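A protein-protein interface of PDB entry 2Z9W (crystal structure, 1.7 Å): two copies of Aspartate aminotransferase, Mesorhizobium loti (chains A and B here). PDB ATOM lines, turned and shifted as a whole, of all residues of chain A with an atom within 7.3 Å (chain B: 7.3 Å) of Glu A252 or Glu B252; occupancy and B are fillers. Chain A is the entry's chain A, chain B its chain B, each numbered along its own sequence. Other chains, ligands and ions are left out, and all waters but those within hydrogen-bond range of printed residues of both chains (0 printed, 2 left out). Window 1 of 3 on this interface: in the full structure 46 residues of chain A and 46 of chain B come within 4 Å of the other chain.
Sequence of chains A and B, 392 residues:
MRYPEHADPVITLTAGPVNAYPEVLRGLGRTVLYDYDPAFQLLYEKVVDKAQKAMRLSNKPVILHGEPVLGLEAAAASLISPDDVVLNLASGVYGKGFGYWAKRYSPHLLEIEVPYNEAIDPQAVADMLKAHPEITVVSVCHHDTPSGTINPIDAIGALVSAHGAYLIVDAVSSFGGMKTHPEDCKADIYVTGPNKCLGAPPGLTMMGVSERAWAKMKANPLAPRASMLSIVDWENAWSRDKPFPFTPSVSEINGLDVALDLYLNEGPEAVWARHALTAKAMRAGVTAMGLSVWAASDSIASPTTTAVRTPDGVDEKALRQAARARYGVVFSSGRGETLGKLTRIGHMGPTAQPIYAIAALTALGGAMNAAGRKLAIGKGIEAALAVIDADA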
ATOM      1  N   VAL A  24      14.135 -10.218  10.118  1.00  0.00           N
ATOM      2  CA  VAL A  24      15.347  -9.511  10.576  1.00  0.00           C
ATOM      3  C   VAL A  24      14.994  -8.044  10.819  1.00  0.00           C
ATOM      4  O   VAL A  24      15.381  -7.471  11.848  1.00  0.00           O
ATOM      5  CB  VAL A  24      16.498  -9.638   9.558  1.00  0.00           C
ATOM      6  CG1 VAL A  24      17.664  -8.685   9.890  1.00  0.00           C
ATOM      7  CG2 VAL A  24      16.993 -11.094   9.499  1.00  0.00           C
ATOM      8  N   GLY A  27      13.284  -7.740  13.904  1.00  0.00           N
ATOM      9  CA  GLY A  27      14.292  -7.980  14.943  1.00  0.00           C
ATOM     10  C   GLY A  27      15.099  -6.725  15.293  1.00  0.00           C
ATOM     11  O   GLY A  27      15.424  -6.488  16.460  1.00  0.00           O
ATOM     12  N   LEU A  28      15.442  -5.936  14.277  1.00  0.00           N
ATOM     13  CA  LEU A  28      16.144  -4.662  14.495  1.00  0.00           C
ATOM     14  C   LEU A  28      15.349  -3.745  15.422  1.00  0.00           C
ATOM     15  O   LEU A  28      15.923  -2.877  16.071  1.00  0.00           O
ATOM     16  CB  LEU A  28      16.392  -3.953  13.158  1.00  0.00           C
ATOM     17  CG  LEU A  28      17.322  -4.680  12.179  1.00  0.00           C
ATOM     18  CD1 LEU A  28      17.317  -3.990  10.795  1.00  0.00           C
ATOM     19  CD2 LEU A  28      18.703  -4.673  12.746  1.00  0.00           C
ATOM     20  N   VAL A  47      24.393 -15.182  20.736  1.00  0.00           N
ATOM     21  CA  VAL A  47      24.592 -14.844  19.308  1.00  0.00           C
ATOM     22  C   VAL A  47      25.938 -15.374  18.824  1.00  0.00           C
ATOM     23  O   VAL A  47      26.039 -15.914  17.729  1.00  0.00           O
ATOM     24  CB  VAL A  47      24.476 -13.313  19.016  1.00  0.00           C
ATOM     25  CG1 VAL A  47      24.927 -12.969  17.588  1.00  0.00           C
ATOM     26  CG2 VAL A  47      23.031 -12.850  19.196  1.00  0.00           C
ATOM     27  N   HIS A  65      32.283  -4.697  15.299  1.00  0.00           N
ATOM     28  CA  HIS A  65      31.143  -3.789  15.173  1.00  0.00           C
ATOM     29  C   HIS A  65      31.304  -2.751  14.079  1.00  0.00           C
ATOM     30  O   HIS A  65      31.207  -1.544  14.290  1.00  0.00           O
ATOM     31  CB  HIS A  65      30.760  -3.261  16.543  1.00  0.00           C
ATOM     32  CG  HIS A  65      30.270  -4.365  17.415  1.00  0.00           C
ATOM     33  ND1 HIS A  65      28.928  -4.620  17.587  1.00  0.00           N
ATOM     34  CD2 HIS A  65      30.931  -5.395  17.997  1.00  0.00           C
ATOM     35  CE1 HIS A  65      28.785  -5.705  18.332  1.00  0.00           C
ATOM     36  NE2 HIS A  65      29.987  -6.197  18.590  1.00  0.00           N
ATOM     37  N   PRO A 194      26.727 -10.604   7.843  1.00  0.00           N
ATOM     38  CA  PRO A 194      25.369 -11.030   7.506  1.00  0.00           C
ATOM     39  C   PRO A 194      24.714 -10.226   6.385  1.00  0.00           C
ATOM     40  O   PRO A 194      23.542 -10.463   6.086  1.00  0.00           O
ATOM     41  CB  PRO A 194      24.623 -10.816   8.819  1.00  0.00           C
ATOM     42  CG  PRO A 194      25.281  -9.584   9.394  1.00  0.00           C
ATOM     43  CD  PRO A 194      26.746  -9.673   8.994  1.00  0.00           C
ATOM     44  N   ALA A 200      20.706  -9.686   6.333  1.00  0.00           N
ATOM     45  CA  ALA A 200      20.664  -8.634   7.374  1.00  0.00           C
ATOM     46  C   ALA A 200      21.343  -7.375   6.809  1.00  0.00           C
ATOM     47  O   ALA A 200      22.054  -7.451   5.812  1.00  0.00           O
ATOM     48  CB  ALA A 200      21.357  -9.106   8.645  1.00  0.00           C
ATOM     49  N   PRO A 201      21.076  -6.192   7.399  1.00  0.00           N
ATOM     50  CA  PRO A 201      21.727  -4.998   6.834  1.00  0.00           C
ATOM     51  C   PRO A 201      23.222  -4.912   7.178  1.00  0.00           C
ATOM     52  O   PRO A 201      23.714  -5.671   8.013  1.00  0.00           O
ATOM     53  CB  PRO A 201      20.963  -3.831   7.485  1.00  0.00           C
ATOM     54  CG  PRO A 201      20.392  -4.377   8.703  1.00  0.00           C
ATOM     55  CD  PRO A 201      20.175  -5.863   8.518  1.00  0.00           C
ATOM     56  N   PRO A 202      23.934  -3.979   6.538  1.00  0.00           N
ATOM     57  CA  PRO A 202      25.357  -3.788   6.834  1.00  0.00           C
ATOM     58  C   PRO A 202      25.582  -3.207   8.225  1.00  0.00           C
ATOM     59  O   PRO A 202      24.842  -2.322   8.657  1.00  0.00           O
ATOM     60  CB  PRO A 202      25.805  -2.777   5.762  1.00  0.00           C
ATOM     61  CG  PRO A 202      24.726  -2.764   4.744  1.00  0.00           C
ATOM     62  CD  PRO A 202      23.470  -3.076   5.464  1.00  0.00           C
ATOM     63  N   GLY A 203      26.598  -3.701   8.921  1.00  0.00           N
ATOM     64  CA  GLY A 203      26.963  -3.132  10.205  1.00  0.00           C
ATOM     65  C   GLY A 203      27.848  -4.002  11.069  1.00  0.00           C
ATOM     66  O   GLY A 203      28.531  -3.480  11.962  1.00  0.00           O
ATOM     67  N   LEU A 204      27.838  -5.320  10.813  1.00  0.00           N
ATOM     68  CA  LEU A 204      28.612  -6.252  11.638  1.00  0.00           C
ATOM     69  C   LEU A 204      29.540  -7.147  10.824  1.00  0.00           C
ATOM     70  O   LEU A 204      29.279  -7.407   9.660  1.00  0.00           O
ATOM     71  CB  LEU A 204      27.679  -7.146  12.448  1.00  0.00           C
ATOM     72  CG  LEU A 204      26.828  -6.430  13.501  1.00  0.00           C
ATOM     73  CD1 LEU A 204      25.894  -7.441  14.163  1.00  0.00           C
ATOM     74  CD2 LEU A 204      27.693  -5.689  14.562  1.00  0.00           C
ATOM     75  N   PRO A 248      28.711  -2.147  21.786  1.00  0.00           N
ATOM     76  CA  PRO A 248      28.312  -2.915  20.600  1.00  0.00           C
ATOM     77  C   PRO A 248      27.079  -2.298  19.897  1.00  0.00           C
ATOM     78  O   PRO A 248      26.296  -1.565  20.534  1.00  0.00           O
ATOM     79  CB  PRO A 248      27.967  -4.299  21.181  1.00  0.00           C
ATOM     80  CG  PRO A 248      27.581  -4.027  22.620  1.00  0.00           C
ATOM     81  CD  PRO A 248      28.511  -2.905  23.038  1.00  0.00           C
ATOM     82  N   SER A 249      26.915  -2.593  18.608  1.00  0.00           N
ATOM     83  CA  SER A 249      25.756  -2.134  17.851  1.00  0.00           C
ATOM     84  C   SER A 249      24.538  -2.982  18.210  1.00  0.00           C
ATOM     85  O   SER A 249      24.207  -3.962  17.523  1.00  0.00           O
ATOM     86  CB  SER A 249      26.058  -2.160  16.345  1.00  0.00           C
ATOM     87  OG  SER A 249      27.203  -1.363  16.062  1.00  0.00           O
ATOM     88  N   VAL A 250      23.883  -2.592  19.299  1.00  0.00           N
ATOM     89  CA  VAL A 250      22.857  -3.423  19.933  1.00  0.00           C
ATOM     90  C   VAL A 250      21.762  -3.850  18.940  1.00  0.00           C
ATOM     91  O   VAL A 250      21.372  -5.031  18.909  1.00  0.00           O
ATOM     92  CB  VAL A 250      22.242  -2.716  21.164  1.00  0.00           C
ATOM     93  CG1 VAL A 250      21.036  -3.491  21.694  1.00  0.00           C
ATOM     94  CG2 VAL A 250      23.310  -2.554  22.255  1.00  0.00           C
ATOM     95  N   SER A 251      21.258  -2.903  18.145  1.00  0.00           N
ATOM     96  CA  SER A 251      20.155  -3.240  17.241  1.00  0.00           C
ATOM     97  C   SER A 251      20.646  -4.174  16.130  1.00  0.00           C
ATOM     98  O   SER A 251      19.942  -5.117  15.764  1.00  0.00           O
ATOM     99  CB  SER A 251      19.459  -1.997  16.678  1.00  0.00           C
ATOM    100  OG  SER A 251      18.864  -1.272  17.757  1.00  0.00           O
ATOM    101  N   GLU A 252      21.859  -3.938  15.630  1.00  0.00           N
ATOM    102  CA  GLU A 252      22.445  -4.847  14.618  1.00  0.00           C
ATOM    103  C   GLU A 252      22.620  -6.263  15.170  1.00  0.00           C
ATOM    104  O   GLU A 252      22.438  -7.256  14.441  1.00  0.00           O
ATOM    105  CB  GLU A 252      23.776  -4.318  14.082  1.00  0.00           C
ATOM    106  CG  GLU A 252      23.721  -2.950  13.424  1.00  0.00           C
ATOM    107  CD  GLU A 252      22.843  -2.913  12.188  1.00  0.00           C
ATOM    108  OE1 GLU A 252      22.771  -3.923  11.437  1.00  0.00           O
ATOM    109  OE2 GLU A 252      22.216  -1.865  11.953  1.00  0.00           O
ATOM    110  N   ILE A 253      22.976  -6.358  16.452  1.00  0.00           N
ATOM    111  CA  ILE A 253      23.072  -7.648  17.131  1.00  0.00           C
ATOM    112  C   ILE A 253      21.714  -8.360  17.173  1.00  0.00           C
ATOM    113  O   ILE A 253      21.628  -9.586  16.943  1.00  0.00           O
ATOM    114  CB  ILE A 253      23.720  -7.496  18.536  1.00  0.00           C
ATOM    115  CG1 ILE A 253      25.235  -7.258  18.388  1.00  0.00           C
ATOM    116  CG2 ILE A 253      23.405  -8.691  19.422  1.00  0.00           C
ATOM    117  CD1 ILE A 253      26.061  -8.522  17.922  1.00  0.00           C
ATOM    118  N   ASN A 254      20.654  -7.591  17.445  1.00  0.00           N
ATOM    119  CA  ASN A 254      19.293  -8.129  17.419  1.00  0.00           C
ATOM    120  C   ASN A 254      18.935  -8.691  16.043  1.00  0.00           C
ATOM    121  O   ASN A 254      18.374  -9.789  15.940  1.00  0.00           O
ATOM    122  CB  ASN A 254      18.267  -7.076  17.895  1.00  0.00           C
ATOM    123  CG  ASN A 254      18.293  -6.874  19.419  1.00  0.00           C
ATOM    124  OD1 ASN A 254      18.163  -5.741  19.927  1.00  0.00           O
ATOM    125  ND2 ASN A 254      18.441  -7.952  20.146  1.00  0.00           N
ATOM    126  N   GLY A 255      19.299  -7.952  14.993  1.00  0.00           N
ATOM    127  CA  GLY A 255      19.085  -8.398  13.605  1.00  0.00           C
ATOM    128  C   GLY A 255      19.877  -9.650  13.310  1.00  0.00           C
ATOM    129  O   GLY A 255      19.367 -10.575  12.685  1.00  0.00           O
ATOM    130  N   LEU A 256      21.124  -9.685  13.782  1.00  0.00           N
ATOM    131  CA  LEU A 256      21.995 -10.832  13.520  1.00  0.00           C
ATOM    132  C   LEU A 256      21.473 -12.093  14.217  1.00  0.00           C
ATOM    133  O   LEU A 256      21.528 -13.195  13.655  1.00  0.00           O
ATOM    134  CB  LEU A 256      23.430 -10.548  13.974  1.00  0.00           C
ATOM    135  CG  LEU A 256      24.436 -11.702  13.805  1.00  0.00           C
ATOM    136  CD1 LEU A 256      24.523 -12.157  12.347  1.00  0.00           C
ATOM    137  CD2 LEU A 256      25.814 -11.290  14.324  1.00  0.00           C
ATOM    138  N   ASP A 257      20.985 -11.920  15.443  1.00  0.00           N
ATOM    139  CA  ASP A 257      20.334 -13.000  16.192  1.00  0.00           C
ATOM    140  C   ASP A 257      19.237 -13.675  15.342  1.00  0.00           C
ATOM    141  O   ASP A 257      19.200 -14.917  15.174  1.00  0.00           O
ATOM    142  CB  ASP A 257      19.761 -12.412  17.501  1.00  0.00           C
ATOM    143  CG  ASP A 257      19.211 -13.469  18.430  1.00  0.00           C
ATOM    144  OD1 ASP A 257      19.877 -14.516  18.603  1.00  0.00           O
ATOM    145  OD2 ASP A 257      18.107 -13.262  18.989  1.00  0.00           O
ATOM    146  N   VAL A 258      18.368 -12.852  14.759  1.00  0.00           N
ATOM    147  CA  VAL A 258      17.287 -13.352  13.906  1.00  0.00           C
ATOM    148  C   VAL A 258      17.811 -13.977  12.616  1.00  0.00           C
ATOM    149  O   VAL A 258      17.366 -15.064  12.225  1.00  0.00           O
ATOM    150  CB  VAL A 258      16.259 -12.249  13.595  1.00  0.00           C
ATOM    151  CG1 VAL A 258      15.179 -12.743  12.587  1.00  0.00           C
ATOM    152  CG2 VAL A 258      15.605 -11.794  14.882  1.00  0.00           C
ATOM    153  N   VAL B  24      11.866   5.325  16.179  1.00  0.00           N
ATOM    154  CA  VAL B  24      13.205   4.988  15.676  1.00  0.00           C
ATOM    155  C   VAL B  24      13.321   3.492  15.455  1.00  0.00           C
ATOM    156  O   VAL B  24      13.808   3.062  14.411  1.00  0.00           O
ATOM    157  CB  VAL B  24      14.333   5.497  16.608  1.00  0.00           C
ATOM    158  CG1 VAL B  24      15.712   4.948  16.164  1.00  0.00           C
ATOM    159  CG2 VAL B  24      14.329   7.027  16.646  1.00  0.00           C
ATOM    160  N   GLY B  27      11.557   2.709  12.406  1.00  0.00           N
ATOM    161  CA  GLY B  27      12.377   3.200  11.306  1.00  0.00           C
ATOM    162  C   GLY B  27      13.513   2.256  10.936  1.00  0.00           C
ATOM    163  O   GLY B  27      13.832   2.119   9.766  1.00  0.00           O
ATOM    164  N   LEU B  28      14.116   1.607  11.935  1.00  0.00           N
ATOM    165  CA  LEU B  28      15.167   0.620  11.687  1.00  0.00           C
ATOM    166  C   LEU B  28      14.635  -0.505  10.778  1.00  0.00           C
ATOM    167  O   LEU B  28      15.403  -1.126  10.041  1.00  0.00           O
ATOM    168  CB  LEU B  28      15.702   0.049  13.017  1.00  0.00           C
ATOM    169  CG  LEU B  28      16.401   1.050  13.966  1.00  0.00           C
ATOM    170  CD1 LEU B  28      16.713   0.400  15.311  1.00  0.00           C
ATOM    171  CD2 LEU B  28      17.674   1.601  13.343  1.00  0.00           C
ATOM    172  N   VAL B  47      19.459  13.042   4.953  1.00  0.00           N
ATOM    173  CA  VAL B  47      19.847  12.779   6.354  1.00  0.00           C
ATOM    174  C   VAL B  47      21.017  13.682   6.788  1.00  0.00           C
ATOM    175  O   VAL B  47      21.014  14.257   7.894  1.00  0.00           O
ATOM    176  CB  VAL B  47      20.186  11.281   6.616  1.00  0.00           C
ATOM    177  CG1 VAL B  47      20.850  11.113   7.999  1.00  0.00           C
ATOM    178  CG2 VAL B  47      18.920  10.446   6.539  1.00  0.00           C
ATOM    179  N   HIS B  65      30.487   5.460   9.832  1.00  0.00           N
ATOM    180  CA  HIS B  65      29.681   4.259  10.035  1.00  0.00           C
ATOM    181  C   HIS B  65      30.230   3.343  11.118  1.00  0.00           C
ATOM    182  O   HIS B  65      30.505   2.153  10.910  1.00  0.00           O
ATOM    183  CB  HIS B  65      29.400   3.612   8.674  1.00  0.00           C
ATOM    184  CG  HIS B  65      28.566   4.503   7.827  1.00  0.00           C
ATOM    185  ND1 HIS B  65      27.199   4.359   7.729  1.00  0.00           N
ATOM    186  CD2 HIS B  65      28.874   5.661   7.191  1.00  0.00           C
ATOM    187  CE1 HIS B  65      26.709   5.356   7.009  1.00  0.00           C
ATOM    188  NE2 HIS B  65      27.704   6.162   6.672  1.00  0.00           N
ATOM    189  N   PRO B 194      23.915   9.601  17.583  1.00  0.00           N
ATOM    190  CA  PRO B 194      22.490   9.582  17.993  1.00  0.00           C
ATOM    191  C   PRO B 194      22.178   8.636  19.163  1.00  0.00           C
ATOM    192  O   PRO B 194      21.017   8.505  19.552  1.00  0.00           O
ATOM    193  CB  PRO B 194      21.787   9.092  16.727  1.00  0.00           C
ATOM    194  CG  PRO B 194      22.817   8.102  16.114  1.00  0.00           C
ATOM    195  CD  PRO B 194      24.202   8.665  16.470  1.00  0.00           C
ATOM    196  N   ALA B 200      18.545   6.890  19.486  1.00  0.00           N
ATOM    197  CA  ALA B 200      18.775   5.828  18.475  1.00  0.00           C
ATOM    198  C   ALA B 200      19.789   4.834  19.031  1.00  0.00           C
ATOM    199  O   ALA B 200      20.482   5.153  19.993  1.00  0.00           O
ATOM    200  CB  ALA B 200      19.282   6.434  17.185  1.00  0.00           C
ATOM    201  N   PRO B 201      19.870   3.611  18.457  1.00  0.00           N
ATOM    202  CA  PRO B 201      20.894   2.689  18.953  1.00  0.00           C
ATOM    203  C   PRO B 201      22.327   3.068  18.542  1.00  0.00           C
ATOM    204  O   PRO B 201      22.522   3.942  17.686  1.00  0.00           O
ATOM    205  CB  PRO B 201      20.508   1.345  18.301  1.00  0.00           C
ATOM    206  CG  PRO B 201      19.783   1.721  17.076  1.00  0.00           C
ATOM    207  CD  PRO B 201      19.045   3.004  17.395  1.00  0.00           C
ATOM    208  N   PRO B 202      23.331   2.387  19.127  1.00  0.00           N
ATOM    209  CA  PRO B 202      24.715   2.657  18.743  1.00  0.00           C
ATOM    210  C   PRO B 202      25.016   2.156  17.356  1.00  0.00           C
ATOM    211  O   PRO B 202      24.540   1.054  16.970  1.00  0.00           O
ATOM    212  CB  PRO B 202      25.532   1.848  19.750  1.00  0.00           C
ATOM    213  CG  PRO B 202      24.561   1.487  20.884  1.00  0.00           C
ATOM    214  CD  PRO B 202      23.236   1.366  20.188  1.00  0.00           C
ATOM    215  N   GLY B 203      25.794   2.934  16.601  1.00  0.00           N
ATOM    216  CA  GLY B 203      26.230   2.484  15.272  1.00  0.00           C
ATOM    217  C   GLY B 203      26.731   3.545  14.315  1.00  0.00           C
ATOM    218  O   GLY B 203      27.455   3.228  13.384  1.00  0.00           O
ATOM    219  N   LEU B 204      26.334   4.805  14.538  1.00  0.00           N
ATOM    220  CA  LEU B 204      26.763   5.918  13.697  1.00  0.00           C
ATOM    221  C   LEU B 204      27.414   7.051  14.471  1.00  0.00           C
ATOM    222  O   LEU B 204      27.168   7.218  15.664  1.00  0.00           O
ATOM    223  CB  LEU B 204      25.583   6.481  12.903  1.00  0.00           C
ATOM    224  CG  LEU B 204      24.906   5.540  11.892  1.00  0.00           C
ATOM    225  CD1 LEU B 204      23.668   6.221  11.342  1.00  0.00           C
ATOM    226  CD2 LEU B 204      25.843   5.092  10.767  1.00  0.00           C
ATOM    227  N   PRO B 248      27.474   1.905   3.606  1.00  0.00           N
ATOM    228  CA  PRO B 248      26.908   2.542   4.785  1.00  0.00           C
ATOM    229  C   PRO B 248      25.957   1.625   5.543  1.00  0.00           C
ATOM    230  O   PRO B 248      25.407   0.683   4.962  1.00  0.00           O
ATOM    231  CB  PRO B 248      26.144   3.747   4.208  1.00  0.00           C
ATOM    232  CG  PRO B 248      25.798   3.351   2.817  1.00  0.00           C
ATOM    233  CD  PRO B 248      27.004   2.537   2.357  1.00  0.00           C
ATOM    234  N   SER B 249      25.802   1.883   6.844  1.00  0.00           N
ATOM    235  CA  SER B 249      24.921   1.078   7.686  1.00  0.00           C
ATOM    236  C   SER B 249      23.486   1.502   7.411  1.00  0.00           C
ATOM    237  O   SER B 249      22.918   2.370   8.088  1.00  0.00           O
ATOM    238  CB  SER B 249      25.309   1.231   9.162  1.00  0.00           C
ATOM    239  OG  SER B 249      26.661   0.808   9.348  1.00  0.00           O
ATOM    240  N   VAL B 250      22.911   0.889   6.381  1.00  0.00           N
ATOM    241  CA  VAL B 250      21.649   1.362   5.806  1.00  0.00           C
ATOM    242  C   VAL B 250      20.520   1.457   6.837  1.00  0.00           C
ATOM    243  O   VAL B 250      19.803   2.465   6.882  1.00  0.00           O
ATOM    244  CB  VAL B 250      21.219   0.510   4.567  1.00  0.00           C
ATOM    245  CG1 VAL B 250      19.804   0.876   4.105  1.00  0.00           C
ATOM    246  CG2 VAL B 250      22.227   0.682   3.392  1.00  0.00           C
ATOM    247  N   SER B 251      20.361   0.417   7.652  1.00  0.00           N
ATOM    248  CA  SER B 251      19.282   0.432   8.643  1.00  0.00           C
ATOM    249  C   SER B 251      19.536   1.480   9.713  1.00  0.00           C
ATOM    250  O   SER B 251      18.600   2.160  10.115  1.00  0.00           O
ATOM    251  CB  SER B 251      19.055  -0.938   9.258  1.00  0.00           C
ATOM    252  OG  SER B 251      18.639  -1.827   8.223  1.00  0.00           O
ATOM    253  N   GLU B 252      20.795   1.645  10.127  1.00  0.00           N
ATOM    254  CA  GLU B 252      21.118   2.713  11.096  1.00  0.00           C
ATOM    255  C   GLU B 252      20.821   4.102  10.533  1.00  0.00           C
ATOM    256  O   GLU B 252      20.420   5.005  11.272  1.00  0.00           O
ATOM    257  CB  GLU B 252      22.576   2.648  11.556  1.00  0.00           C
ATOM    258  CG  GLU B 252      22.972   1.319  12.198  1.00  0.00           C
ATOM    259  CD  GLU B 252      22.226   1.022  13.479  1.00  0.00           C
ATOM    260  OE1 GLU B 252      21.875   1.963  14.216  1.00  0.00           O
ATOM    261  OE2 GLU B 252      21.981  -0.165  13.764  1.00  0.00           O
ATOM    262  N   ILE B 253      21.044   4.273   9.236  1.00  0.00           N
ATOM    263  CA  ILE B 253      20.713   5.531   8.568  1.00  0.00           C
ATOM    264  C   ILE B 253      19.200   5.778   8.605  1.00  0.00           C
ATOM    265  O   ILE B 253      18.757   6.898   8.869  1.00  0.00           O
ATOM    266  CB  ILE B 253      21.258   5.557   7.124  1.00  0.00           C
ATOM    267  CG1 ILE B 253      22.789   5.751   7.129  1.00  0.00           C
ATOM    268  CG2 ILE B 253      20.543   6.642   6.287  1.00  0.00           C
ATOM    269  CD1 ILE B 253      23.289   7.152   7.613  1.00  0.00           C
ATOM    270  N   ASN B 254      18.413   4.728   8.369  1.00  0.00           N
ATOM    271  CA  ASN B 254      16.954   4.830   8.501  1.00  0.00           C
ATOM    272  C   ASN B 254      16.548   5.236   9.914  1.00  0.00           C
ATOM    273  O   ASN B 254      15.653   6.059  10.100  1.00  0.00           O
ATOM    274  CB  ASN B 254      16.268   3.511   8.105  1.00  0.00           C
ATOM    275  CG  ASN B 254      16.274   3.261   6.590  1.00  0.00           C
ATOM    276  OD1 ASN B 254      16.468   2.119   6.134  1.00  0.00           O
ATOM    277  ND2 ASN B 254      16.044   4.306   5.812  1.00  0.00           N
ATOM    278  N   GLY B 255      17.215   4.677  10.912  1.00  0.00           N
ATOM    279  CA  GLY B 255      16.960   5.081  12.295  1.00  0.00           C
ATOM    280  C   GLY B 255      17.323   6.535  12.573  1.00  0.00           C
ATOM    281  O   GLY B 255      16.565   7.261  13.224  1.00  0.00           O
ATOM    282  N   LEU B 256      18.489   6.947  12.083  1.00  0.00           N
ATOM    283  CA  LEU B 256      18.968   8.309  12.256  1.00  0.00           C
ATOM    284  C   LEU B 256      17.998   9.300  11.602  1.00  0.00           C
ATOM    285  O   LEU B 256      17.714  10.368  12.156  1.00  0.00           O
ATOM    286  CB  LEU B 256      20.383   8.481  11.682  1.00  0.00           C
ATOM    287  CG  LEU B 256      20.994   9.892  11.814  1.00  0.00           C
ATOM    288  CD1 LEU B 256      21.033  10.333  13.274  1.00  0.00           C
ATOM    289  CD2 LEU B 256      22.400   9.898  11.211  1.00  0.00           C
ATOM    290  N   ASP B 257      17.489   8.940  10.428  1.00  0.00           N
ATOM    291  CA  ASP B 257      16.518   9.771   9.703  1.00  0.00           C
ATOM    292  C   ASP B 257      15.326  10.106  10.602  1.00  0.00           C
ATOM    293  O   ASP B 257      14.947  11.275  10.754  1.00  0.00           O
ATOM    294  CB  ASP B 257      16.079   9.005   8.456  1.00  0.00           C
ATOM    295  CG  ASP B 257      15.201   9.822   7.526  1.00  0.00           C
ATOM    296  OD1 ASP B 257      15.521  11.011   7.250  1.00  0.00           O
ATOM    297  OD2 ASP B 257      14.217   9.238   7.024  1.00  0.00           O
ATOM    298  N   VAL B 258      14.769   9.069  11.229  1.00  0.00           N
ATOM    299  CA  VAL B 258      13.647   9.209  12.146  1.00  0.00           C
ATOM    300  C   VAL B 258      14.066  10.014  13.381  1.00  0.00           C
ATOM    301  O   VAL B 258      13.353  10.930  13.783  1.00  0.00           O
ATOM    302  CB  VAL B 258      13.055   7.835  12.561  1.00  0.00           C
ATOM    303  CG1 VAL B 258      11.978   7.995  13.661  1.00  0.00           C
ATOM    304  CG2 VAL B 258      12.461   7.139  11.344  1.00  0.00           C
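O of Leu A28 touches CD1 of Leu B28, at 3.5 Å.
Leu A28 touches Ser B251.
Pro A201 touches Ser B251 (CG to OG, 3.1 Å).
Pro A202 touches Pro B248 (CG to O, 3.5 Å).
Pro A202 touches Ser B249.
Pro A248 touches Pro B202 (O to CG, 3.5 Å).
CA of Ser A249 touches O of Pro B202, 3.5 Å away.
OG of Ser A251 touches CD1 of Leu B28 (3.7 Å).
Ser A251 touches Pro B201.
A ring nitrogen (ND1) of His A65 sits at hydrogen-bond distance from the backbone NH of Ser A249 (3.0 Å).
A ring nitrogen (ND1) of His B65 lies within hydrogen-bond range of the backbone NH (N) of Ser B249 (3.0 Å).
Leu B28 touches its own counterpart, Leu A28.
Leu A28 touches Ser B251, and with the chains exchanged Ser A251 touches Leu B28.
Pro A201 touches Ser B251, and with the chains exchanged Ser A251 touches Pro B201.
Pro A202 touches Pro B248, and with the chains exchanged Pro A248 touches Pro B202.
Positions printed for both chains: 24, 27, 28, 47, 65, 194, 200, 201, 202, 203, 204, 248, 249, 250, 251, 252, 253, 254, 255, 256, 257 and 258.
Of the 10 pairs that touch across the chains among the printed residues, 10 have their exchanged pair printed and touching as well.
Glu A252 touches just one residue of chain B: Glu B252 (2.5 Å).
Glu B252 touches just one residue of chain A: Glu A252.
Of the printed residues of chain B, Pro A201 touches Ser B251 (3.1 Å).
Of the printed residues of chain B, Ser A249 touches Pro B202.
Of the printed residues of chain B, Pro A248 touches Pro B202.
Ala A200 touches none of the printed residues of chain B.
Asp B257 touches none of the printed residues of chain A.
The nearest residue of chain B that does not touch Glu A252 is Ser B251 (4.3 Å).
OE2 of Glu A252 lies close to OE2 of Glu B252, 2.5 Å away.
Along chain A the printed residues that touch a printed residue of chain B span positions 28 to 252.
Of the 22 printed residues of chain B, 7 touch a printed residue of chain A.
Hydrophobic or aromatic side chains of chain B within 4 Å of the printed part of chain A: Leu B28, Pro B201 and Pro B202.
Among the printed residues, no Asp or Glu carboxylate lies within 4 Å of a Lys or Arg side-chain nitrogen of the other chain.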
